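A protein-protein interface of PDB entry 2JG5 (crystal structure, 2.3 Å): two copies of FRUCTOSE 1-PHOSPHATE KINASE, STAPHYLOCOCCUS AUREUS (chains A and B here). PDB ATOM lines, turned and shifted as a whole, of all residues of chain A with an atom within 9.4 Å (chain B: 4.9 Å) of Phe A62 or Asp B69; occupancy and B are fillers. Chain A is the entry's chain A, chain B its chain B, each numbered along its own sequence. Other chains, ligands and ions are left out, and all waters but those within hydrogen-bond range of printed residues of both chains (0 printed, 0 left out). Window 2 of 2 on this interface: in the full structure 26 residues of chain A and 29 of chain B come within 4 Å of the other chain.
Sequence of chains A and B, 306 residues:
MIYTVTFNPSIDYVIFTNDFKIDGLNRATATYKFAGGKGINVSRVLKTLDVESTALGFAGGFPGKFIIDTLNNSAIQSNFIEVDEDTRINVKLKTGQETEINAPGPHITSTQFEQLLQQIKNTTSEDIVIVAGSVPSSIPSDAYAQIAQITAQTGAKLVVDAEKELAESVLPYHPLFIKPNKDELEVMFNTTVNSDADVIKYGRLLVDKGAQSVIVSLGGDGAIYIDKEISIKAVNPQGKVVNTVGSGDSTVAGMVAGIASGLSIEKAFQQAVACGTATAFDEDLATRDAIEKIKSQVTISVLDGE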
ATOM      1  N   ILE A  11     -13.040   2.161 -17.203  1.00  0.00           N
ATOM      2  CA  ILE A  11     -13.715   0.941 -17.575  1.00  0.00           C
ATOM      3  C   ILE A  11     -14.963   1.390 -18.325  1.00  0.00           C
ATOM      4  O   ILE A  11     -15.747   2.225 -17.847  1.00  0.00           O
ATOM      5  CB  ILE A  11     -14.055   0.044 -16.371  1.00  0.00           C
ATOM      6  CG1 ILE A  11     -12.782  -0.280 -15.598  1.00  0.00           C
ATOM      7  CG2 ILE A  11     -14.733  -1.265 -16.838  1.00  0.00           C
ATOM      8  CD1 ILE A  11     -13.008  -1.036 -14.315  1.00  0.00           C
ATOM      9  N   LYS A  33     -17.054  -5.508 -20.473  1.00  0.00           N
ATOM     10  CA  LYS A  33     -16.211  -4.436 -19.981  1.00  0.00           C
ATOM     11  C   LYS A  33     -14.964  -4.361 -20.808  1.00  0.00           C
ATOM     12  O   LYS A  33     -14.416  -5.390 -21.197  1.00  0.00           O
ATOM     13  CB  LYS A  33     -15.776  -4.734 -18.545  1.00  0.00           C
ATOM     14  CG  LYS A  33     -16.866  -4.689 -17.517  1.00  0.00           C
ATOM     15  CD  LYS A  33     -16.264  -4.864 -16.130  1.00  0.00           C
ATOM     16  CE  LYS A  33     -17.315  -5.211 -15.138  1.00  0.00           C
ATOM     17  NZ  LYS A  33     -17.833  -6.580 -15.406  1.00  0.00           N
ATOM     18  N   ALA A  59      -4.080   5.630 -12.696  1.00  0.00           N
ATOM     19  CA  ALA A  59      -4.941   4.518 -12.276  1.00  0.00           C
ATOM     20  C   ALA A  59      -4.977   4.338 -10.757  1.00  0.00           C
ATOM     21  O   ALA A  59      -4.000   4.612 -10.059  1.00  0.00           O
ATOM     22  CB  ALA A  59      -4.553   3.229 -12.971  1.00  0.00           C
ATOM     23  N   GLY A  60      -6.120   3.876 -10.259  1.00  0.00           N
ATOM     24  CA  GLY A  60      -6.319   3.698  -8.835  1.00  0.00           C
ATOM     25  C   GLY A  60      -7.401   2.688  -8.525  1.00  0.00           C
ATOM     26  O   GLY A  60      -8.307   2.459  -9.330  1.00  0.00           O
ATOM     27  N   GLY A  61      -7.290   2.098  -7.338  1.00  0.00           N
ATOM     28  CA  GLY A  61      -8.206   1.086  -6.865  1.00  0.00           C
ATOM     29  C   GLY A  61      -8.193  -0.157  -7.725  1.00  0.00           C
ATOM     30  O   GLY A  61      -7.236  -0.422  -8.467  1.00  0.00           O
ATOM     31  N   PHE A  62      -9.273  -0.918  -7.630  1.00  0.00           N
ATOM     32  CA  PHE A  62      -9.396  -2.140  -8.396  1.00  0.00           C
ATOM     33  C   PHE A  62      -9.869  -1.890  -9.837  1.00  0.00           C
ATOM     34  O   PHE A  62      -9.467  -2.612 -10.750  1.00  0.00           O
ATOM     35  CB  PHE A  62     -10.244  -3.150  -7.637  1.00  0.00           C
ATOM     36  CG  PHE A  62      -9.583  -3.654  -6.369  1.00  0.00           C
ATOM     37  CD1 PHE A  62      -8.511  -4.558  -6.429  1.00  0.00           C
ATOM     38  CD2 PHE A  62     -10.028  -3.234  -5.117  1.00  0.00           C
ATOM     39  CE1 PHE A  62      -7.898  -5.032  -5.262  1.00  0.00           C
ATOM     40  CE2 PHE A  62      -9.419  -3.701  -3.951  1.00  0.00           C
ATOM     41  CZ  PHE A  62      -8.351  -4.604  -4.027  1.00  0.00           C
ATOM     42  N   PRO A  63     -10.699  -0.851 -10.055  1.00  0.00           N
ATOM     43  CA  PRO A  63     -10.871  -0.381 -11.421  1.00  0.00           C
ATOM     44  C   PRO A  63      -9.539  -0.086 -12.106  1.00  0.00           C
ATOM     45  O   PRO A  63      -9.432  -0.250 -13.320  1.00  0.00           O
ATOM     46  CB  PRO A  63     -11.654   0.919 -11.236  1.00  0.00           C
ATOM     47  CG  PRO A  63     -12.455   0.680 -10.031  1.00  0.00           C
ATOM     48  CD  PRO A  63     -11.538  -0.082  -9.116  1.00  0.00           C
ATOM     49  N   GLY A  64      -8.538   0.335 -11.327  1.00  0.00           N
ATOM     50  CA  GLY A  64      -7.202   0.637 -11.849  1.00  0.00           C
ATOM     51  C   GLY A  64      -6.488  -0.624 -12.292  1.00  0.00           C
ATOM     52  O   GLY A  64      -5.985  -0.698 -13.413  1.00  0.00           O
ATOM     53  N   LYS A  65      -6.467  -1.612 -11.398  1.00  0.00           N
ATOM     54  CA  LYS A  65      -5.906  -2.925 -11.657  1.00  0.00           C
ATOM     55  C   LYS A  65      -6.510  -3.568 -12.907  1.00  0.00           C
ATOM     56  O   LYS A  65      -5.786  -4.125 -13.734  1.00  0.00           O
ATOM     57  CB  LYS A  65      -6.117  -3.843 -10.442  1.00  0.00           C
ATOM     58  CG  LYS A  65      -5.578  -3.303  -9.108  1.00  0.00           C
ATOM     59  CD  LYS A  65      -4.047  -3.296  -9.060  1.00  0.00           C
ATOM     60  CE  LYS A  65      -3.519  -3.142  -7.629  1.00  0.00           C
ATOM     61  NZ  LYS A  65      -2.175  -3.809  -7.454  1.00  0.00           N
ATOM     62  N   PHE A  66      -7.831  -3.486 -13.048  1.00  0.00           N
ATOM     63  CA  PHE A  66      -8.514  -4.048 -14.215  1.00  0.00           C
ATOM     64  C   PHE A  66      -7.924  -3.548 -15.535  1.00  0.00           C
ATOM     65  O   PHE A  66      -7.724  -4.326 -16.477  1.00  0.00           O
ATOM     66  CB  PHE A  66     -10.013  -3.730 -14.176  1.00  0.00           C
ATOM     67  CG  PHE A  66     -10.750  -4.125 -15.435  1.00  0.00           C
ATOM     68  CD1 PHE A  66     -11.288  -5.399 -15.569  1.00  0.00           C
ATOM     69  CD2 PHE A  66     -10.897  -3.221 -16.488  1.00  0.00           C
ATOM     70  CE1 PHE A  66     -11.965  -5.770 -16.733  1.00  0.00           C
ATOM     71  CE2 PHE A  66     -11.576  -3.584 -17.656  1.00  0.00           C
ATOM     72  CZ  PHE A  66     -12.113  -4.859 -17.773  1.00  0.00           C
ATOM     73  N   ILE A  67      -7.673  -2.242 -15.592  1.00  0.00           N
ATOM     74  CA  ILE A  67      -7.089  -1.617 -16.768  1.00  0.00           C
ATOM     75  C   ILE A  67      -5.668  -2.128 -17.038  1.00  0.00           C
ATOM     76  O   ILE A  67      -5.305  -2.407 -18.195  1.00  0.00           O
ATOM     77  CB  ILE A  67      -7.120  -0.085 -16.644  1.00  0.00           C
ATOM     78  CG1 ILE A  67      -8.576   0.397 -16.710  1.00  0.00           C
ATOM     79  CG2 ILE A  67      -6.265   0.565 -17.730  1.00  0.00           C
ATOM     80  CD1 ILE A  67      -8.729   1.901 -16.784  1.00  0.00           C
ATOM     81  N   ILE A  68      -4.877  -2.268 -15.976  1.00  0.00           N
ATOM     82  CA  ILE A  68      -3.531  -2.801 -16.121  1.00  0.00           C
ATOM     83  C   ILE A  68      -3.566  -4.263 -16.598  1.00  0.00           C
ATOM     84  O   ILE A  68      -2.875  -4.618 -17.568  1.00  0.00           O
ATOM     85  CB  ILE A  68      -2.697  -2.636 -14.837  1.00  0.00           C
ATOM     86  CG1 ILE A  68      -2.782  -1.188 -14.324  1.00  0.00           C
ATOM     87  CG2 ILE A  68      -1.249  -3.026 -15.096  1.00  0.00           C
ATOM     88  CD1 ILE A  68      -2.241  -0.973 -12.908  1.00  0.00           C
ATOM     89  N   ASP A  69      -4.389  -5.093 -15.959  1.00  0.00           N
ATOM     90  CA  ASP A  69      -4.500  -6.505 -16.353  1.00  0.00           C
ATOM     91  C   ASP A  69      -5.055  -6.678 -17.769  1.00  0.00           C
ATOM     92  O   ASP A  69      -4.583  -7.531 -18.522  1.00  0.00           O
ATOM     93  CB  ASP A  69      -5.334  -7.305 -15.338  1.00  0.00           C
ATOM     94  CG  ASP A  69      -4.665  -7.403 -13.973  1.00  0.00           C
ATOM     95  OD1 ASP A  69      -3.666  -6.691 -13.730  1.00  0.00           O
ATOM     96  OD2 ASP A  69      -5.135  -8.194 -13.132  1.00  0.00           O
ATOM     97  N   THR A  70      -6.044  -5.857 -18.121  1.00  0.00           N
ATOM     98  CA  THR A  70      -6.619  -5.845 -19.466  1.00  0.00           C
ATOM     99  C   THR A  70      -5.565  -5.496 -20.509  1.00  0.00           C
ATOM    100  O   THR A  70      -5.428  -6.200 -21.515  1.00  0.00           O
ATOM    101  CB  THR A  70      -7.837  -4.884 -19.555  1.00  0.00           C
ATOM    102  OG1 THR A  70      -8.926  -5.438 -18.806  1.00  0.00           O
ATOM    103  CG2 THR A  70      -8.297  -4.683 -20.993  1.00  0.00           C
ATOM    104  N   GLU A  82      -0.225   5.549  -9.676  1.00  0.00           N
ATOM    105  CA  GLU A  82      -1.243   5.110  -8.718  1.00  0.00           C
ATOM    106  C   GLU A  82      -1.841   6.325  -8.031  1.00  0.00           C
ATOM    107  O   GLU A  82      -1.129   7.116  -7.392  1.00  0.00           O
ATOM    108  CB  GLU A  82      -0.661   4.129  -7.684  1.00  0.00           C
ATOM    109  CG  GLU A  82      -1.711   3.400  -6.801  1.00  0.00           C
ATOM    110  CD  GLU A  82      -1.109   2.766  -5.552  1.00  0.00           C
ATOM    111  OE1 GLU A  82      -0.885   1.535  -5.553  1.00  0.00           O
ATOM    112  OE2 GLU A  82      -0.847   3.492  -4.564  1.00  0.00           O
ATOM    113  N   VAL A  83      -3.146   6.489  -8.196  1.00  0.00           N
ATOM    114  CA  VAL A  83      -3.886   7.515  -7.467  1.00  0.00           C
ATOM    115  C   VAL A  83      -4.737   6.859  -6.360  1.00  0.00           C
ATOM    116  O   VAL A  83      -4.949   5.645  -6.373  1.00  0.00           O
ATOM    117  CB  VAL A  83      -4.713   8.438  -8.419  1.00  0.00           C
ATOM    118  CG1 VAL A  83      -3.789   9.089  -9.444  1.00  0.00           C
ATOM    119  CG2 VAL A  83      -5.786   7.660  -9.143  1.00  0.00           C
ATOM    120  N   ASP A  84      -5.198   7.670  -5.408  1.00  0.00           N
ATOM    121  CA  ASP A  84      -5.820   7.195  -4.170  1.00  0.00           C
ATOM    122  C   ASP A  84      -7.327   6.906  -4.299  1.00  0.00           C
ATOM    123  O   ASP A  84      -7.946   6.377  -3.374  1.00  0.00           O
ATOM    124  CB  ASP A  84      -5.585   8.212  -3.043  1.00  0.00           C
ATOM    125  CG  ASP A  84      -4.117   8.562  -2.863  1.00  0.00           C
ATOM    126  OD1 ASP A  84      -3.275   7.638  -2.939  1.00  0.00           O
ATOM    127  OD2 ASP A  84      -3.808   9.761  -2.638  1.00  0.00           O
ATOM    128  N   GLU A  85      -7.910   7.255  -5.439  1.00  0.00           N
ATOM    129  CA  GLU A  85      -9.318   6.943  -5.699  1.00  0.00           C
ATOM    130  C   GLU A  85      -9.488   6.063  -6.946  1.00  0.00           C
ATOM    131  O   GLU A  85      -8.577   5.951  -7.777  1.00  0.00           O
ATOM    132  CB  GLU A  85     -10.140   8.231  -5.842  1.00  0.00           C
ATOM    133  CG  GLU A  85     -10.193   9.074  -4.578  1.00  0.00           C
ATOM    134  CD  GLU A  85     -11.185  10.206  -4.669  1.00  0.00           C
ATOM    135  OE1 GLU A  85     -11.873  10.339  -5.705  1.00  0.00           O
ATOM    136  OE2 GLU A  85     -11.270  10.973  -3.694  1.00  0.00           O
ATOM    137  N   ASP A  86     -10.673   5.465  -7.075  1.00  0.00           N
ATOM    138  CA  ASP A  86     -10.957   4.524  -8.153  1.00  0.00           C
ATOM    139  C   ASP A  86     -10.973   5.128  -9.549  1.00  0.00           C
ATOM    140  O   ASP A  86     -11.588   6.175  -9.787  1.00  0.00           O
ATOM    141  CB  ASP A  86     -12.277   3.804  -7.894  1.00  0.00           C
ATOM    142  CG  ASP A  86     -12.178   2.801  -6.766  1.00  0.00           C
ATOM    143  OD1 ASP A  86     -11.061   2.545  -6.268  1.00  0.00           O
ATOM    144  OD2 ASP A  86     -13.222   2.265  -6.371  1.00  0.00           O
ATOM    145  N   THR A  87     -10.294   4.444 -10.465  1.00  0.00           N
ATOM    146  CA  THR A  87     -10.407   4.712 -11.895  1.00  0.00           C
ATOM    147  C   THR A  87     -11.896   4.668 -12.226  1.00  0.00           C
ATOM    148  O   THR A  87     -12.631   3.837 -11.677  1.00  0.00           O
ATOM    149  CB  THR A  87      -9.614   3.673 -12.712  1.00  0.00           C
ATOM    150  OG1 THR A  87      -8.208   3.913 -12.543  1.00  0.00           O
ATOM    151  CG2 THR A  87      -9.949   3.757 -14.187  1.00  0.00           C
ATOM    152  N   ARG A  88     -12.354   5.575 -13.083  1.00  0.00           N
ATOM    153  CA  ARG A  88     -13.803   5.687 -13.330  1.00  0.00           C
ATOM    154  C   ARG A  88     -14.391   4.515 -14.097  1.00  0.00           C
ATOM    155  O   ARG A  88     -13.680   3.821 -14.843  1.00  0.00           O
ATOM    156  CB  ARG A  88     -14.169   7.005 -14.015  1.00  0.00           C
ATOM    157  CG  ARG A  88     -13.489   7.241 -15.342  1.00  0.00           C
ATOM    158  CD  ARG A  88     -14.030   8.479 -16.006  1.00  0.00           C
ATOM    159  NE  ARG A  88     -13.230   8.821 -17.168  1.00  0.00           N
ATOM    160  CZ  ARG A  88     -13.632   9.572 -18.185  1.00  0.00           C
ATOM    161  NH1 ARG A  88     -14.863  10.067 -18.220  1.00  0.00           N
ATOM    162  NH2 ARG A  88     -12.794   9.819 -19.179  1.00  0.00           N
ATOM    163  N   ILE A  89     -15.692   4.318 -13.882  1.00  0.00           N
ATOM    164  CA  ILE A  89     -16.501   3.385 -14.647  1.00  0.00           C
ATOM    165  C   ILE A  89     -17.559   4.161 -15.428  1.00  0.00           C
ATOM    166  O   ILE A  89     -18.487   4.733 -14.859  1.00  0.00           O
ATOM    167  CB  ILE A  89     -17.195   2.292 -13.768  1.00  0.00           C
ATOM    168  CG1 ILE A  89     -16.153   1.487 -12.954  1.00  0.00           C
ATOM    169  CG2 ILE A  89     -17.973   1.359 -14.669  1.00  0.00           C
ATOM    170  CD1 ILE A  89     -16.756   0.500 -11.901  1.00  0.00           C
ATOM    171  N   PHE B  62     -12.327  -7.677 -10.617  1.00  0.00           N
ATOM    172  CA  PHE B  62     -12.095  -6.454  -9.826  1.00  0.00           C
ATOM    173  C   PHE B  62     -13.273  -6.084  -8.906  1.00  0.00           C
ATOM    174  O   PHE B  62     -13.040  -5.577  -7.811  1.00  0.00           O
ATOM    175  CB  PHE B  62     -11.661  -5.251 -10.697  1.00  0.00           C
ATOM    176  CG  PHE B  62     -12.816  -4.440 -11.256  1.00  0.00           C
ATOM    177  CD1 PHE B  62     -13.496  -3.517 -10.453  1.00  0.00           C
ATOM    178  CD2 PHE B  62     -13.220  -4.602 -12.587  1.00  0.00           C
ATOM    179  CE1 PHE B  62     -14.565  -2.781 -10.957  1.00  0.00           C
ATOM    180  CE2 PHE B  62     -14.291  -3.868 -13.105  1.00  0.00           C
ATOM    181  CZ  PHE B  62     -14.966  -2.954 -12.286  1.00  0.00           C
ATOM    182  N   LYS B  65     -12.955  -8.045  -5.844  1.00  0.00           N
ATOM    183  CA  LYS B  65     -11.891  -7.395  -5.092  1.00  0.00           C
ATOM    184  C   LYS B  65     -12.436  -6.233  -4.270  1.00  0.00           C
ATOM    185  O   LYS B  65     -12.200  -6.156  -3.062  1.00  0.00           O
ATOM    186  CB  LYS B  65     -10.802  -6.882  -6.033  1.00  0.00           C
ATOM    187  CG  LYS B  65     -10.051  -7.929  -6.829  1.00  0.00           C
ATOM    188  CD  LYS B  65      -9.194  -8.814  -5.946  1.00  0.00           C
ATOM    189  CE  LYS B  65      -8.366  -9.797  -6.783  1.00  0.00           C
ATOM    190  NZ  LYS B  65      -7.756 -10.868  -5.921  1.00  0.00           N
ATOM    191  N   PHE B  66     -13.186  -5.352  -4.936  1.00  0.00           N
ATOM    192  CA  PHE B  66     -13.784  -4.182  -4.304  1.00  0.00           C
ATOM    193  C   PHE B  66     -14.586  -4.533  -3.054  1.00  0.00           C
ATOM    194  O   PHE B  66     -14.500  -3.833  -2.049  1.00  0.00           O
ATOM    195  CB  PHE B  66     -14.681  -3.427  -5.292  1.00  0.00           C
ATOM    196  CG  PHE B  66     -15.545  -2.370  -4.639  1.00  0.00           C
ATOM    197  CD1 PHE B  66     -15.066  -1.078  -4.454  1.00  0.00           C
ATOM    198  CD2 PHE B  66     -16.835  -2.678  -4.192  1.00  0.00           C
ATOM    199  CE1 PHE B  66     -15.855  -0.112  -3.840  1.00  0.00           C
ATOM    200  CE2 PHE B  66     -17.629  -1.715  -3.578  1.00  0.00           C
ATOM    201  CZ  PHE B  66     -17.137  -0.434  -3.403  1.00  0.00           C
ATOM    202  N   ILE B  67     -15.376  -5.607  -3.138  1.00  0.00           N
ATOM    203  CA  ILE B  67     -16.289  -5.979  -2.062  1.00  0.00           C
ATOM    204  C   ILE B  67     -15.502  -6.524  -0.871  1.00  0.00           C
ATOM    205  O   ILE B  67     -15.764  -6.148   0.270  1.00  0.00           O
ATOM    206  CB  ILE B  67     -17.386  -6.985  -2.538  1.00  0.00           C
ATOM    207  CG1 ILE B  67     -18.309  -6.328  -3.566  1.00  0.00           C
ATOM    208  CG2 ILE B  67     -18.201  -7.499  -1.351  1.00  0.00           C
ATOM    209  CD1 ILE B  67     -19.356  -7.263  -4.105  1.00  0.00           C
ATOM    210  N   ILE B  68     -14.537  -7.397  -1.155  1.00  0.00           N
ATOM    211  CA  ILE B  68     -13.602  -7.902  -0.149  1.00  0.00           C
ATOM    212  C   ILE B  68     -12.954  -6.732   0.616  1.00  0.00           C
ATOM    213  O   ILE B  68     -12.925  -6.718   1.849  1.00  0.00           O
ATOM    214  CB  ILE B  68     -12.533  -8.837  -0.800  1.00  0.00           C
ATOM    215  CG1 ILE B  68     -13.192 -10.118  -1.326  1.00  0.00           C
ATOM    216  CG2 ILE B  68     -11.369  -9.163   0.186  1.00  0.00           C
ATOM    217  CD1 ILE B  68     -12.435 -10.787  -2.473  1.00  0.00           C
ATOM    218  N   ASP B  69     -12.470  -5.748  -0.135  1.00  0.00           N
ATOM    219  CA  ASP B  69     -11.871  -4.545   0.416  1.00  0.00           C
ATOM    220  C   ASP B  69     -12.782  -3.697   1.278  1.00  0.00           C
ATOM    221  O   ASP B  69     -12.375  -3.204   2.333  1.00  0.00           O
ATOM    222  CB  ASP B  69     -11.368  -3.670  -0.721  1.00  0.00           C
ATOM    223  CG  ASP B  69      -9.892  -3.629  -0.779  1.00  0.00           C
ATOM    224  OD1 ASP B  69      -9.325  -2.547  -0.509  1.00  0.00           O
ATOM    225  OD2 ASP B  69      -9.308  -4.694  -1.068  1.00  0.00           O
ATOM    226  N   THR B  70     -13.998  -3.491   0.785  1.00  0.00           N
ATOM    227  CA  THR B  70     -15.015  -2.724   1.472  1.00  0.00           C
ATOM    228  C   THR B  70     -15.250  -3.338   2.837  1.00  0.00           C
ATOM    229  O   THR B  70     -15.352  -2.624   3.829  1.00  0.00           O
ATOM    230  CB  THR B  70     -16.323  -2.732   0.667  1.00  0.00           C
ATOM    231  OG1 THR B  70     -16.066  -2.234  -0.651  1.00  0.00           O
ATOM    232  CG2 THR B  70     -17.372  -1.864   1.330  1.00  0.00           C
ATOM    233  N   LEU B  71     -15.309  -4.669   2.864  1.00  0.00           N
ATOM    234  CA  LEU B  71     -15.576  -5.448   4.071  1.00  0.00           C
ATOM    235  C   LEU B  71     -14.403  -5.424   5.051  1.00  0.00           C
ATOM    236  O   LEU B  71     -14.617  -5.334   6.256  1.00  0.00           O
ATOM    237  CB  LEU B  71     -15.970  -6.885   3.700  1.00  0.00           C
ATOM    238  CG  LEU B  71     -17.296  -7.096   2.956  1.00  0.00           C
ATOM    239  CD1 LEU B  71     -17.551  -8.585   2.723  1.00  0.00           C
ATOM    240  CD2 LEU B  71     -18.481  -6.457   3.691  1.00  0.00           C
ATOM    241  N   ASN B  72     -13.175  -5.493   4.522  1.00  0.00           N
ATOM    242  CA  ASN B  72     -11.948  -5.264   5.297  1.00  0.00           C
ATOM    243  C   ASN B  72     -11.949  -3.881   5.944  1.00  0.00           C
ATOM    244  O   ASN B  72     -11.522  -3.718   7.096  1.00  0.00           O
ATOM    245  CB  ASN B  72     -10.690  -5.366   4.408  1.00  0.00           C
ATOM    246  CG  ASN B  72     -10.388  -6.787   3.945  1.00  0.00           C
ATOM    247  OD1 ASN B  72     -10.623  -7.760   4.660  1.00  0.00           O
ATOM    248  ND2 ASN B  72      -9.834  -6.904   2.742  1.00  0.00           N
ATOM    249  N   ASN B  73     -12.395  -2.884   5.176  1.00  0.00           N
ATOM    250  CA  ASN B  73     -12.436  -1.502   5.637  1.00  0.00           C
ATOM    251  C   ASN B  73     -13.453  -1.354   6.756  1.00  0.00           C
ATOM    252  O   ASN B  73     -13.359  -0.430   7.564  1.00  0.00           O
ATOM    253  CB  ASN B  73     -12.759  -0.535   4.488  1.00  0.00           C
ATOM    254  CG  ASN B  73     -11.583  -0.326   3.525  1.00  0.00           C
ATOM    255  OD1 ASN B  73     -10.424  -0.609   3.844  1.00  0.00           O
ATOM    256  ND2 ASN B  73     -11.889   0.192   2.338  1.00  0.00           N
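The backbone carbonyl oxygen (O) of Phe B66 sits at hydrogen-bond distance from the side-chain hydroxyl (OG1) of Thr B70 (2.6 Å). The backbone carbonyl oxygen of Asp B69 sits close to the side-chain amide nitrogen of Asn B73. The side-chain hydroxyl (OG1) of Thr A70 is in hydrogen-bond range of the backbone carbonyl oxygen (O) of Phe A66 (2.8 Å). The backbone NH of Ile A11 lies within hydrogen-bond range of the backbone carbonyl oxygen of Arg A88, 3.0 Å away.
Phe A62 touches just these residues of chain B: Phe B62 (3.4 Å), Lys B65 (3.3 Å), Phe B66 (3.8 Å) and Asp B69 (3.1 Å). Gly A64 touches none of the printed residues of chain B. Of the printed residues of chain B, Phe A66 touches Phe B62. Ile A68 touches none of the printed residues of chain B. Of the printed residues of chain A, Lys B65 touches Phe A62. No residue of chain A comes within 4 Å of Thr B70. The nearest printed residue of chain B that does not touch Ile A11 is Phe B66 (9.5 Å).
Among the printed residues, pairs that only touch across the chains: Ile A11 with Phe B62 (3.3 Å), Lys A33 with Phe B62 (3.7 Å), Phe A62 with Phe B62 (3.4 Å), Phe A62 with Lys B65 (3.3 Å), Phe A62 with Phe B66 (3.8 Å), Phe A62 with Asp B69 (3.1 Å), Pro A63 with Phe B62 (3.9 Å), Phe A66 with Phe B62 (3.6 Å) and Ile A89 with Phe B62 (3.9 Å).
Phe A62 touches its own counterpart, Phe B62. Phe A62 touches Lys B65, but with the chains exchanged Lys A65 does not touch Phe B62 (5.7 Å). Phe A62 touches Phe B66, and with the chains exchanged Phe A66 touches Phe B62. Phe A62 touches Asp B69, but with the chains exchanged Asp A69 does not touch Phe B62 (7.6 Å). Positions printed for both chains: 62, 65, 66, 67, 68, 69 and 70. Of the 9 pairs that touch across the chains among the printed residues, 3 have their exchanged pair printed and touching as well.
Printed residues of chain B that touch a printed residue of chain A: Phe B62, Lys B65, Phe B66 and Asp B69. Hydrophobic or aromatic side chains of chain B that line the printed part of chain A: Phe B62. Of the 22 printed residues of chain A, 6 touch a printed residue of chain B. Hydrophobic or aromatic side chains of chain A that line the printed part of chain B: Ile A11, Phe A62, Phe A66 and Ile A89. Among the printed residues, 9 pairs touch across the chains. Among the printed residues, no Asp or Glu carboxylate lies within 4 Å of a Lys or Arg side-chain nitrogen of the other chain.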
